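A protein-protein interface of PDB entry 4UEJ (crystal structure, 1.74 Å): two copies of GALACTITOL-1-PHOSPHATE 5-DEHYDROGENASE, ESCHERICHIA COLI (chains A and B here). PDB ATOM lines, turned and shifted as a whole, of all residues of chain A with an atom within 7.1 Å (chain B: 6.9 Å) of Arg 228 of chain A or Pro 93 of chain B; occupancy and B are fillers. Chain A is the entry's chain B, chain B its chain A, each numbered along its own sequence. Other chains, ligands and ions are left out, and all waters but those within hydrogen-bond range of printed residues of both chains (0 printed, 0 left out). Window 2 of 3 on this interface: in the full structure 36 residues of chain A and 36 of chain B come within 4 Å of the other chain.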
ATOM      1  N   ASN A 163     -21.775  25.335  -0.652  1.00  0.00           N
ATOM      2  CA  ASN A 163     -20.928  25.943   0.350  1.00  0.00           C
ATOM      3  C   ASN A 163     -21.321  27.397   0.506  1.00  0.00           C
ATOM      4  O   ASN A 163     -20.906  28.257  -0.278  1.00  0.00           O
ATOM      5  CB  ASN A 163     -19.456  25.810  -0.029  1.00  0.00           C
ATOM      6  CG  ASN A 163     -18.975  24.367   0.025  1.00  0.00           C
ATOM      7  OD1 ASN A 163     -19.146  23.685   1.036  1.00  0.00           O
ATOM      8  ND2 ASN A 163     -18.345  23.909  -1.055  1.00  0.00           N
ATOM      9  N   GLN A 221      -9.530  33.521   1.593  1.00  0.00           N
ATOM     10  CA  GLN A 221      -9.590  32.659   0.420  1.00  0.00           C
ATOM     11  C   GLN A 221      -8.712  31.430   0.641  1.00  0.00           C
ATOM     12  O   GLN A 221      -9.013  30.338   0.160  1.00  0.00           O
ATOM     13  CB  GLN A 221      -9.166  33.419  -0.850  1.00  0.00           C
ATOM     14  CG  GLN A 221      -9.664  32.778  -2.119  1.00  0.00           C
ATOM     15  CD  GLN A 221      -9.307  33.568  -3.369  1.00  0.00           C
ATOM     16  OE1 GLN A 221      -8.583  34.565  -3.311  1.00  0.00           O
ATOM     17  NE2 GLN A 221      -9.807  33.112  -4.509  1.00  0.00           N
ATOM     18  N   VAL A 223      -8.209  29.909   3.537  1.00  0.00           N
ATOM     19  CA  VAL A 223      -8.942  28.992   4.388  1.00  0.00           C
ATOM     20  C   VAL A 223     -10.040  28.290   3.593  1.00  0.00           C
ATOM     21  O   VAL A 223     -10.311  27.099   3.785  1.00  0.00           O
ATOM     22  CB  VAL A 223      -9.543  29.724   5.596  1.00  0.00           C
ATOM     23  CG1 VAL A 223     -10.408  28.785   6.419  1.00  0.00           C
ATOM     24  CG2 VAL A 223      -8.427  30.310   6.449  1.00  0.00           C
ATOM     25  N   LEU A 224     -10.651  29.033   2.680  1.00  0.00           N
ATOM     26  CA  LEU A 224     -11.760  28.530   1.890  1.00  0.00           C
ATOM     27  C   LEU A 224     -11.352  27.560   0.782  1.00  0.00           C
ATOM     28  O   LEU A 224     -12.230  27.051   0.100  1.00  0.00           O
ATOM     29  CB  LEU A 224     -12.520  29.699   1.254  1.00  0.00           C
ATOM     30  CG  LEU A 224     -13.354  30.549   2.213  1.00  0.00           C
ATOM     31  CD1 LEU A 224     -13.856  31.825   1.530  1.00  0.00           C
ATOM     32  CD2 LEU A 224     -14.510  29.718   2.701  1.00  0.00           C
ATOM     33  N   ARG A 225     -10.046  27.320   0.592  1.00  0.00           N
ATOM     34  CA  ARG A 225      -9.588  26.489  -0.525  1.00  0.00           C
ATOM     35  C   ARG A 225     -10.362  25.176  -0.678  1.00  0.00           C
ATOM     36  O   ARG A 225     -10.803  24.851  -1.787  1.00  0.00           O
ATOM     37  CB  ARG A 225      -8.090  26.175  -0.395  1.00  0.00           C
ATOM     38  CG  ARG A 225      -7.174  27.323  -0.802  1.00  0.00           C
ATOM     39  CD  ARG A 225      -7.261  27.614  -2.295  1.00  0.00           C
ATOM     40  NE  ARG A 225      -6.504  26.655  -3.099  1.00  0.00           N
ATOM     41  CZ  ARG A 225      -6.471  26.663  -4.430  1.00  0.00           C
ATOM     42  NH1 ARG A 225      -7.156  27.577  -5.105  1.00  0.00           N
ATOM     43  NH2 ARG A 225      -5.762  25.756  -5.089  1.00  0.00           N
ATOM     44  N   GLU A 226     -10.529  24.434   0.419  1.00  0.00           N
ATOM     45  CA  GLU A 226     -11.205  23.135   0.373  1.00  0.00           C
ATOM     46  C   GLU A 226     -12.680  23.269   0.001  1.00  0.00           C
ATOM     47  O   GLU A 226     -13.292  22.323  -0.485  1.00  0.00           O
ATOM     48  CB  GLU A 226     -11.105  22.406   1.721  1.00  0.00           C
ATOM     49  CG  GLU A 226      -9.718  22.301   2.318  1.00  0.00           C
ATOM     50  CD  GLU A 226      -9.753  21.874   3.788  1.00  0.00           C
ATOM     51  OE1 GLU A 226     -10.171  22.683   4.647  1.00  0.00           O
ATOM     52  OE2 GLU A 226      -9.368  20.727   4.083  1.00  0.00           O
ATOM     53  N   LEU A 227     -13.246  24.446   0.237  1.00  0.00           N
ATOM     54  CA  LEU A 227     -14.674  24.670   0.036  1.00  0.00           C
ATOM     55  C   LEU A 227     -14.898  25.676  -1.082  1.00  0.00           C
ATOM     56  O   LEU A 227     -15.912  26.367  -1.105  1.00  0.00           O
ATOM     57  CB  LEU A 227     -15.333  25.171   1.325  1.00  0.00           C
ATOM     58  CG  LEU A 227     -15.217  24.249   2.541  1.00  0.00           C
ATOM     59  CD1 LEU A 227     -15.981  24.824   3.715  1.00  0.00           C
ATOM     60  CD2 LEU A 227     -15.722  22.854   2.199  1.00  0.00           C
ATOM     61  N   ARG A 228     -13.953  25.762  -2.014  1.00  0.00           N
ATOM     62  CA  ARG A 228     -14.026  26.836  -3.009  1.00  0.00           C
ATOM     63  C   ARG A 228     -15.044  26.569  -4.106  1.00  0.00           C
ATOM     64  O   ARG A 228     -15.455  27.504  -4.811  1.00  0.00           O
ATOM     65  CB  ARG A 228     -12.649  27.105  -3.640  1.00  0.00           C
ATOM     66  CG  ARG A 228     -12.083  26.009  -4.530  1.00  0.00           C
ATOM     67  CD  ARG A 228     -10.668  26.425  -4.963  1.00  0.00           C
ATOM     68  NE  ARG A 228      -9.979  25.470  -5.829  1.00  0.00           N
ATOM     69  CZ  ARG A 228      -9.308  24.401  -5.394  1.00  0.00           C
ATOM     70  NH1 ARG A 228      -9.262  24.116  -4.098  1.00  0.00           N
ATOM     71  NH2 ARG A 228      -8.690  23.603  -6.259  1.00  0.00           N
ATOM     72  N   PHE A 229     -15.473  25.318  -4.257  1.00  0.00           N
ATOM     73  CA  PHE A 229     -16.430  25.028  -5.331  1.00  0.00           C
ATOM     74  C   PHE A 229     -17.874  25.088  -4.835  1.00  0.00           C
ATOM     75  O   PHE A 229     -18.128  24.988  -3.638  1.00  0.00           O
ATOM     76  CB  PHE A 229     -16.145  23.665  -5.958  1.00  0.00           C
ATOM     77  CG  PHE A 229     -14.824  23.591  -6.678  1.00  0.00           C
ATOM     78  CD1 PHE A 229     -14.677  24.134  -7.947  1.00  0.00           C
ATOM     79  CD2 PHE A 229     -13.736  22.982  -6.092  1.00  0.00           C
ATOM     80  CE1 PHE A 229     -13.455  24.058  -8.618  1.00  0.00           C
ATOM     81  CE2 PHE A 229     -12.516  22.901  -6.757  1.00  0.00           C
ATOM     82  CZ  PHE A 229     -12.381  23.436  -8.017  1.00  0.00           C
ATOM     83  N   ASN A 230     -18.802  25.280  -5.771  1.00  0.00           N
ATOM     84  CA  ASN A 230     -20.230  25.330  -5.483  1.00  0.00           C
ATOM     85  C   ASN A 230     -20.583  26.283  -4.342  1.00  0.00           C
ATOM     86  O   ASN A 230     -21.421  25.983  -3.492  1.00  0.00           O
ATOM     87  CB  ASN A 230     -20.747  23.930  -5.182  1.00  0.00           C
ATOM     88  CG  ASN A 230     -20.567  22.990  -6.363  1.00  0.00           C
ATOM     89  OD1 ASN A 230     -21.136  23.213  -7.429  1.00  0.00           O
ATOM     90  ND2 ASN A 230     -19.773  21.939  -6.178  1.00  0.00           N
ATOM     91  N   GLN A 231     -19.934  27.438  -4.336  1.00  0.00           N
ATOM     92  CA  GLN A 231     -20.217  28.462  -3.350  1.00  0.00           C
ATOM     93  C   GLN A 231     -21.442  29.277  -3.672  1.00  0.00           C
ATOM     94  O   GLN A 231     -21.718  29.587  -4.839  1.00  0.00           O
ATOM     95  CB  GLN A 231     -19.044  29.412  -3.211  1.00  0.00           C
ATOM     96  CG  GLN A 231     -17.847  28.782  -2.555  1.00  0.00           C
ATOM     97  CD  GLN A 231     -16.737  29.768  -2.336  1.00  0.00           C
ATOM     98  OE1 GLN A 231     -16.763  30.883  -2.873  1.00  0.00           O
ATOM     99  NE2 GLN A 231     -15.758  29.379  -1.528  1.00  0.00           N
ATOM    100  N   ILE A 249     -12.974  36.996  -2.350  1.00  0.00           N
ATOM    101  CA  ILE A 249     -12.814  35.697  -1.708  1.00  0.00           C
ATOM    102  C   ILE A 249     -13.432  34.586  -2.532  1.00  0.00           C
ATOM    103  O   ILE A 249     -13.158  33.411  -2.299  1.00  0.00           O
ATOM    104  CB  ILE A 249     -13.426  35.678  -0.276  1.00  0.00           C
ATOM    105  CG1 ILE A 249     -14.947  35.821  -0.342  1.00  0.00           C
ATOM    106  CG2 ILE A 249     -12.805  36.786   0.567  1.00  0.00           C
ATOM    107  CD1 ILE A 249     -15.646  35.775   1.035  1.00  0.00           C
ATOM    108  N   ALA A 250     -14.241  34.949  -3.524  1.00  0.00           N
ATOM    109  CA  ALA A 250     -15.063  33.949  -4.196  1.00  0.00           C
ATOM    110  C   ALA A 250     -14.250  32.863  -4.890  1.00  0.00           C
ATOM    111  O   ALA A 250     -13.163  33.109  -5.431  1.00  0.00           O
ATOM    112  CB  ALA A 250     -15.998  34.622  -5.207  1.00  0.00           C
ATOM    113  N   GLY A 251     -14.811  31.664  -4.895  1.00  0.00           N
ATOM    114  CA  GLY A 251     -14.200  30.536  -5.557  1.00  0.00           C
ATOM    115  C   GLY A 251     -14.682  30.497  -6.990  1.00  0.00           C
ATOM    116  O   GLY A 251     -15.463  31.354  -7.410  1.00  0.00           O
ATOM    117  N   PRO A 252     -14.208  29.511  -7.749  1.00  0.00           N
ATOM    118  CA  PRO A 252     -14.570  29.409  -9.168  1.00  0.00           C
ATOM    119  C   PRO A 252     -16.068  29.146  -9.350  1.00  0.00           C
ATOM    120  O   PRO A 252     -16.673  28.316  -8.646  1.00  0.00           O
ATOM    121  CB  PRO A 252     -13.724  28.231  -9.675  1.00  0.00           C
ATOM    122  CG  PRO A 252     -13.229  27.548  -8.486  1.00  0.00           C
ATOM    123  CD  PRO A 252     -13.167  28.546  -7.377  1.00  0.00           C
ATOM    124  N   HIS A 253     -16.652  29.900 -10.278  1.00  0.00           N
ATOM    125  CA  HIS A 253     -18.081  29.865 -10.597  1.00  0.00           C
ATOM    126  C   HIS A 253     -19.002  30.060  -9.396  1.00  0.00           C
ATOM    127  O   HIS A 253     -20.141  29.620  -9.420  1.00  0.00           O
ATOM    128  CB  HIS A 253     -18.416  28.558 -11.308  1.00  0.00           C
ATOM    129  CG  HIS A 253     -17.824  28.471 -12.676  1.00  0.00           C
ATOM    130  ND1 HIS A 253     -18.549  28.740 -13.814  1.00  0.00           N
ATOM    131  CD2 HIS A 253     -16.565  28.192 -13.089  1.00  0.00           C
ATOM    132  CE1 HIS A 253     -17.771  28.608 -14.874  1.00  0.00           C
ATOM    133  NE2 HIS A 253     -16.561  28.275 -14.463  1.00  0.00           N
ATOM    134  N   ALA A 254     -18.518  30.745  -8.364  1.00  0.00           N
ATOM    135  CA  ALA A 254     -19.363  31.055  -7.232  1.00  0.00           C
ATOM    136  C   ALA A 254     -20.571  31.871  -7.647  1.00  0.00           C
ATOM    137  O   ALA A 254     -20.515  32.670  -8.581  1.00  0.00           O
ATOM    138  CB  ALA A 254     -18.574  31.800  -6.149  1.00  0.00           C
ATOM    139  N   CYS B  89      -3.982  22.551 -17.653  1.00  0.00           N
ATOM    140  CA  CYS B  89      -3.139  21.465 -17.150  1.00  0.00           C
ATOM    141  C   CYS B  89      -3.871  20.122 -17.210  1.00  0.00           C
ATOM    142  O   CYS B  89      -3.230  19.059 -17.266  1.00  0.00           O
ATOM    143  CB  CYS B  89      -2.670  21.759 -15.716  1.00  0.00           C
ATOM    144  SG  CYS B  89      -3.869  21.378 -14.395  1.00  0.00           S
ATOM    145  N   THR B  91      -5.420  18.498 -15.006  1.00  0.00           N
ATOM    146  CA  THR B  91      -5.295  17.595 -13.861  1.00  0.00           C
ATOM    147  C   THR B  91      -5.587  18.242 -12.505  1.00  0.00           C
ATOM    148  O   THR B  91      -5.548  17.561 -11.488  1.00  0.00           O
ATOM    149  CB  THR B  91      -3.885  16.974 -13.791  1.00  0.00           C
ATOM    150  OG1 THR B  91      -2.918  18.005 -13.560  1.00  0.00           O
ATOM    151  CG2 THR B  91      -3.557  16.240 -15.091  1.00  0.00           C
ATOM    152  N   CYS B  92      -5.868  19.542 -12.489  1.00  0.00           N
ATOM    153  CA  CYS B  92      -6.242  20.219 -11.240  1.00  0.00           C
ATOM    154  C   CYS B  92      -7.751  20.089 -11.044  1.00  0.00           C
ATOM    155  O   CYS B  92      -8.456  19.728 -11.981  1.00  0.00           O
ATOM    156  CB  CYS B  92      -5.833  21.687 -11.268  1.00  0.00           C
ATOM    157  SG  CYS B  92      -6.788  22.679 -12.442  1.00  0.00           S
ATOM    158  N   PRO B  93      -8.251  20.364  -9.824  1.00  0.00           N
ATOM    159  CA  PRO B  93      -9.690  20.206  -9.586  1.00  0.00           C
ATOM    160  C   PRO B  93     -10.561  21.038 -10.519  1.00  0.00           C
ATOM    161  O   PRO B  93     -11.589  20.538 -10.961  1.00  0.00           O
ATOM    162  CB  PRO B  93      -9.855  20.670  -8.134  1.00  0.00           C
ATOM    163  CG  PRO B  93      -8.549  20.355  -7.506  1.00  0.00           C
ATOM    164  CD  PRO B  93      -7.521  20.647  -8.573  1.00  0.00           C
ATOM    165  N   GLU B  94     -10.159  22.274 -10.806  1.00  0.00           N
ATOM    166  CA  GLU B  94     -10.906  23.115 -11.738  1.00  0.00           C
ATOM    167  C   GLU B  94     -11.006  22.451 -13.117  1.00  0.00           C
ATOM    168  O   GLU B  94     -12.085  22.374 -13.696  1.00  0.00           O
ATOM    169  CB  GLU B  94     -10.254  24.495 -11.852  1.00  0.00           C
ATOM    170  CG  GLU B  94     -10.593  25.470 -10.722  1.00  0.00           C
ATOM    171  CD  GLU B  94      -9.746  25.266  -9.468  1.00  0.00           C
ATOM    172  OE1 GLU B  94      -9.010  24.256  -9.385  1.00  0.00           O
ATOM    173  OE2 GLU B  94      -9.820  26.125  -8.562  1.00  0.00           O
ATOM    174  N   CYS B  95      -9.881  21.960 -13.633  1.00  0.00           N
ATOM    175  CA  CYS B  95      -9.879  21.326 -14.958  1.00  0.00           C
ATOM    176  C   CYS B  95     -10.763  20.089 -14.967  1.00  0.00           C
ATOM    177  O   CYS B  95     -11.499  19.854 -15.914  1.00  0.00           O
ATOM    178  CB  CYS B  95      -8.465  20.940 -15.397  1.00  0.00           C
ATOM    179  SG  CYS B  95      -7.456  22.290 -16.046  1.00  0.00           S
ATOM    180  N   LEU B  96     -10.701  19.299 -13.898  1.00  0.00           N
ATOM    181  CA  LEU B  96     -11.497  18.076 -13.833  1.00  0.00           C
ATOM    182  C   LEU B  96     -12.989  18.389 -13.755  1.00  0.00           C
ATOM    183  O   LEU B  96     -13.824  17.526 -14.022  1.00  0.00           O
ATOM    184  CB  LEU B  96     -11.068  17.216 -12.641  1.00  0.00           C
ATOM    185  CG  LEU B  96      -9.622  16.703 -12.721  1.00  0.00           C
ATOM    186  CD1 LEU B  96      -9.250  15.968 -11.444  1.00  0.00           C
ATOM    187  CD2 LEU B  96      -9.401  15.805 -13.943  1.00  0.00           C
ATOM    188  N   LYS B  97     -13.322  19.629 -13.410  1.00  0.00           N
ATOM    189  CA  LYS B  97     -14.720  20.054 -13.409  1.00  0.00           C
ATOM    190  C   LYS B  97     -15.112  20.735 -14.717  1.00  0.00           C
ATOM    191  O   LYS B  97     -16.265  21.126 -14.900  1.00  0.00           O
ATOM    192  CB  LYS B  97     -14.995  20.983 -12.231  1.00  0.00           C
ATOM    193  CG  LYS B  97     -15.165  20.243 -10.909  1.00  0.00           C
ATOM    194  CD  LYS B  97     -15.452  21.199  -9.765  1.00  0.00           C
ATOM    195  CE  LYS B  97     -15.644  20.453  -8.447  1.00  0.00           C
ATOM    196  NZ  LYS B  97     -16.966  19.768  -8.375  1.00  0.00           N
ATOM    197  N   GLY B  98     -14.155  20.865 -15.631  1.00  0.00           N
ATOM    198  CA  GLY B  98     -14.416  21.520 -16.899  1.00  0.00           C
ATOM    199  C   GLY B  98     -14.264  23.027 -16.810  1.00  0.00           C
ATOM    200  O   GLY B  98     -14.630  23.751 -17.734  1.00  0.00           O
ATOM    201  N   PHE B  99     -13.714  23.497 -15.694  1.00  0.00           N
ATOM    202  CA  PHE B  99     -13.456  24.913 -15.499  1.00  0.00           C
ATOM    203  C   PHE B  99     -12.061  25.284 -16.002  1.00  0.00           C
ATOM    204  O   PHE B  99     -11.199  25.670 -15.218  1.00  0.00           O
ATOM    205  CB  PHE B  99     -13.587  25.274 -14.019  1.00  0.00           C
ATOM    206  CG  PHE B  99     -14.947  24.994 -13.439  1.00  0.00           C
ATOM    207  CD1 PHE B  99     -16.061  24.871 -14.258  1.00  0.00           C
ATOM    208  CD2 PHE B  99     -15.112  24.872 -12.075  1.00  0.00           C
ATOM    209  CE1 PHE B  99     -17.310  24.625 -13.729  1.00  0.00           C
ATOM    210  CE2 PHE B  99     -16.360  24.633 -11.533  1.00  0.00           C
ATOM    211  CZ  PHE B  99     -17.460  24.502 -12.359  1.00  0.00           C
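Among the printed residues, pairs that only touch across the chains: His 253 of chain A with Phe 99 of chain B, Arg 228 of chain A with Pro 93 of chain B, Phe 229 of chain A with Glu 94 of chain B, Phe 229 of chain A with Lys 97 of chain B, Pro 252 of chain A with Glu 94 of chain B, Phe 229 of chain A with Pro 93 of chain B and Phe 229 of chain A with Phe 99 of chain B.
Arg 228 of chain A touches two residues of chain B. Printed residues of chain B within 4 Å of Phe 229 of chain A: Pro 93 (3.7 Å), Glu 94 (3.5 Å), Lys 97 (3.5 Å) and Phe 99 (3.9 Å). Printed residues of chain B within 4 Å of His 253 of chain A: Phe 99. Pro 93 of chain B touches just these residues of chain A: Arg 228 (3.5 Å) and Phe 229 (3.7 Å). Of the printed residues of chain A, Glu 94 of chain B touches Arg 228 (2.8 Å), Phe 229 (3.5 Å) and Pro 252 (3.7 Å). Leu 96 of chain B touches none of the printed residues of chain A. Printed residues of chain A within 4 Å of Lys 97 of chain B: Phe 229 (3.5 Å). Printed residues of chain A within 4 Å of Phe 99 of chain B: Phe 229 (3.9 Å) and His 253 (3.4 Å). The nearest residue of chain B that does not touch Arg 228 of chain A is Cys 92 of chain B (6.0 Å). The nearest residue of chain A that does not touch Pro 93 of chain B is Arg 225 of chain A (6.4 Å). The nearest printed residue of chain B that does not touch His 253 of chain A is Gly 98 of chain B (5.9 Å).
The guanidinium group of Arg 228 of chain A lies within salt-bridge range of the side-chain carboxylate of Glu 94 of chain B.
The backbone carbonyl oxygen (O) of Arg 225 of chain A sits at hydrogen-bond distance from the guanidinium group (NH1) of Arg 228 of chain A. ND2 of Asn 163 of chain A is in hydrogen-bond range of O of Phe 229 of chain A (2.8 Å). SG of Cys 92 of chain B lies close to N of Glu 94 of chain B, at 3.8 Å. O of Glu 94 of chain B is in hydrogen-bond range of N of Phe 99 of chain B (2.8 Å).
No position is printed for both chains. Of the 8 pairs that touch across the chains among the printed residues, none has its exchanged pair printed and touching as well.
Of the 17 printed residues of chain A, 4 touch a printed residue of chain B. Printed residues of chain A that touch a printed residue of chain B: Arg 228, Phe 229, Pro 252 and His 253. Hydrophobic or aromatic side chains of chain A within 4 Å of the printed part of chain B: Phe 229, Pro 252 and His 253. Of the 10 printed residues of chain B, 4 touch a printed residue of chain A. Printed residues of chain B that touch a printed residue of chain A: Pro 93, Glu 94, Lys 97 and Phe 99. Among the printed residues, Asp or Glu carboxylates within 4 Å of a Lys or Arg side-chain nitrogen of the other chain: Arg 228 of chain A with Glu 94 of chain B (2.8 Å).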
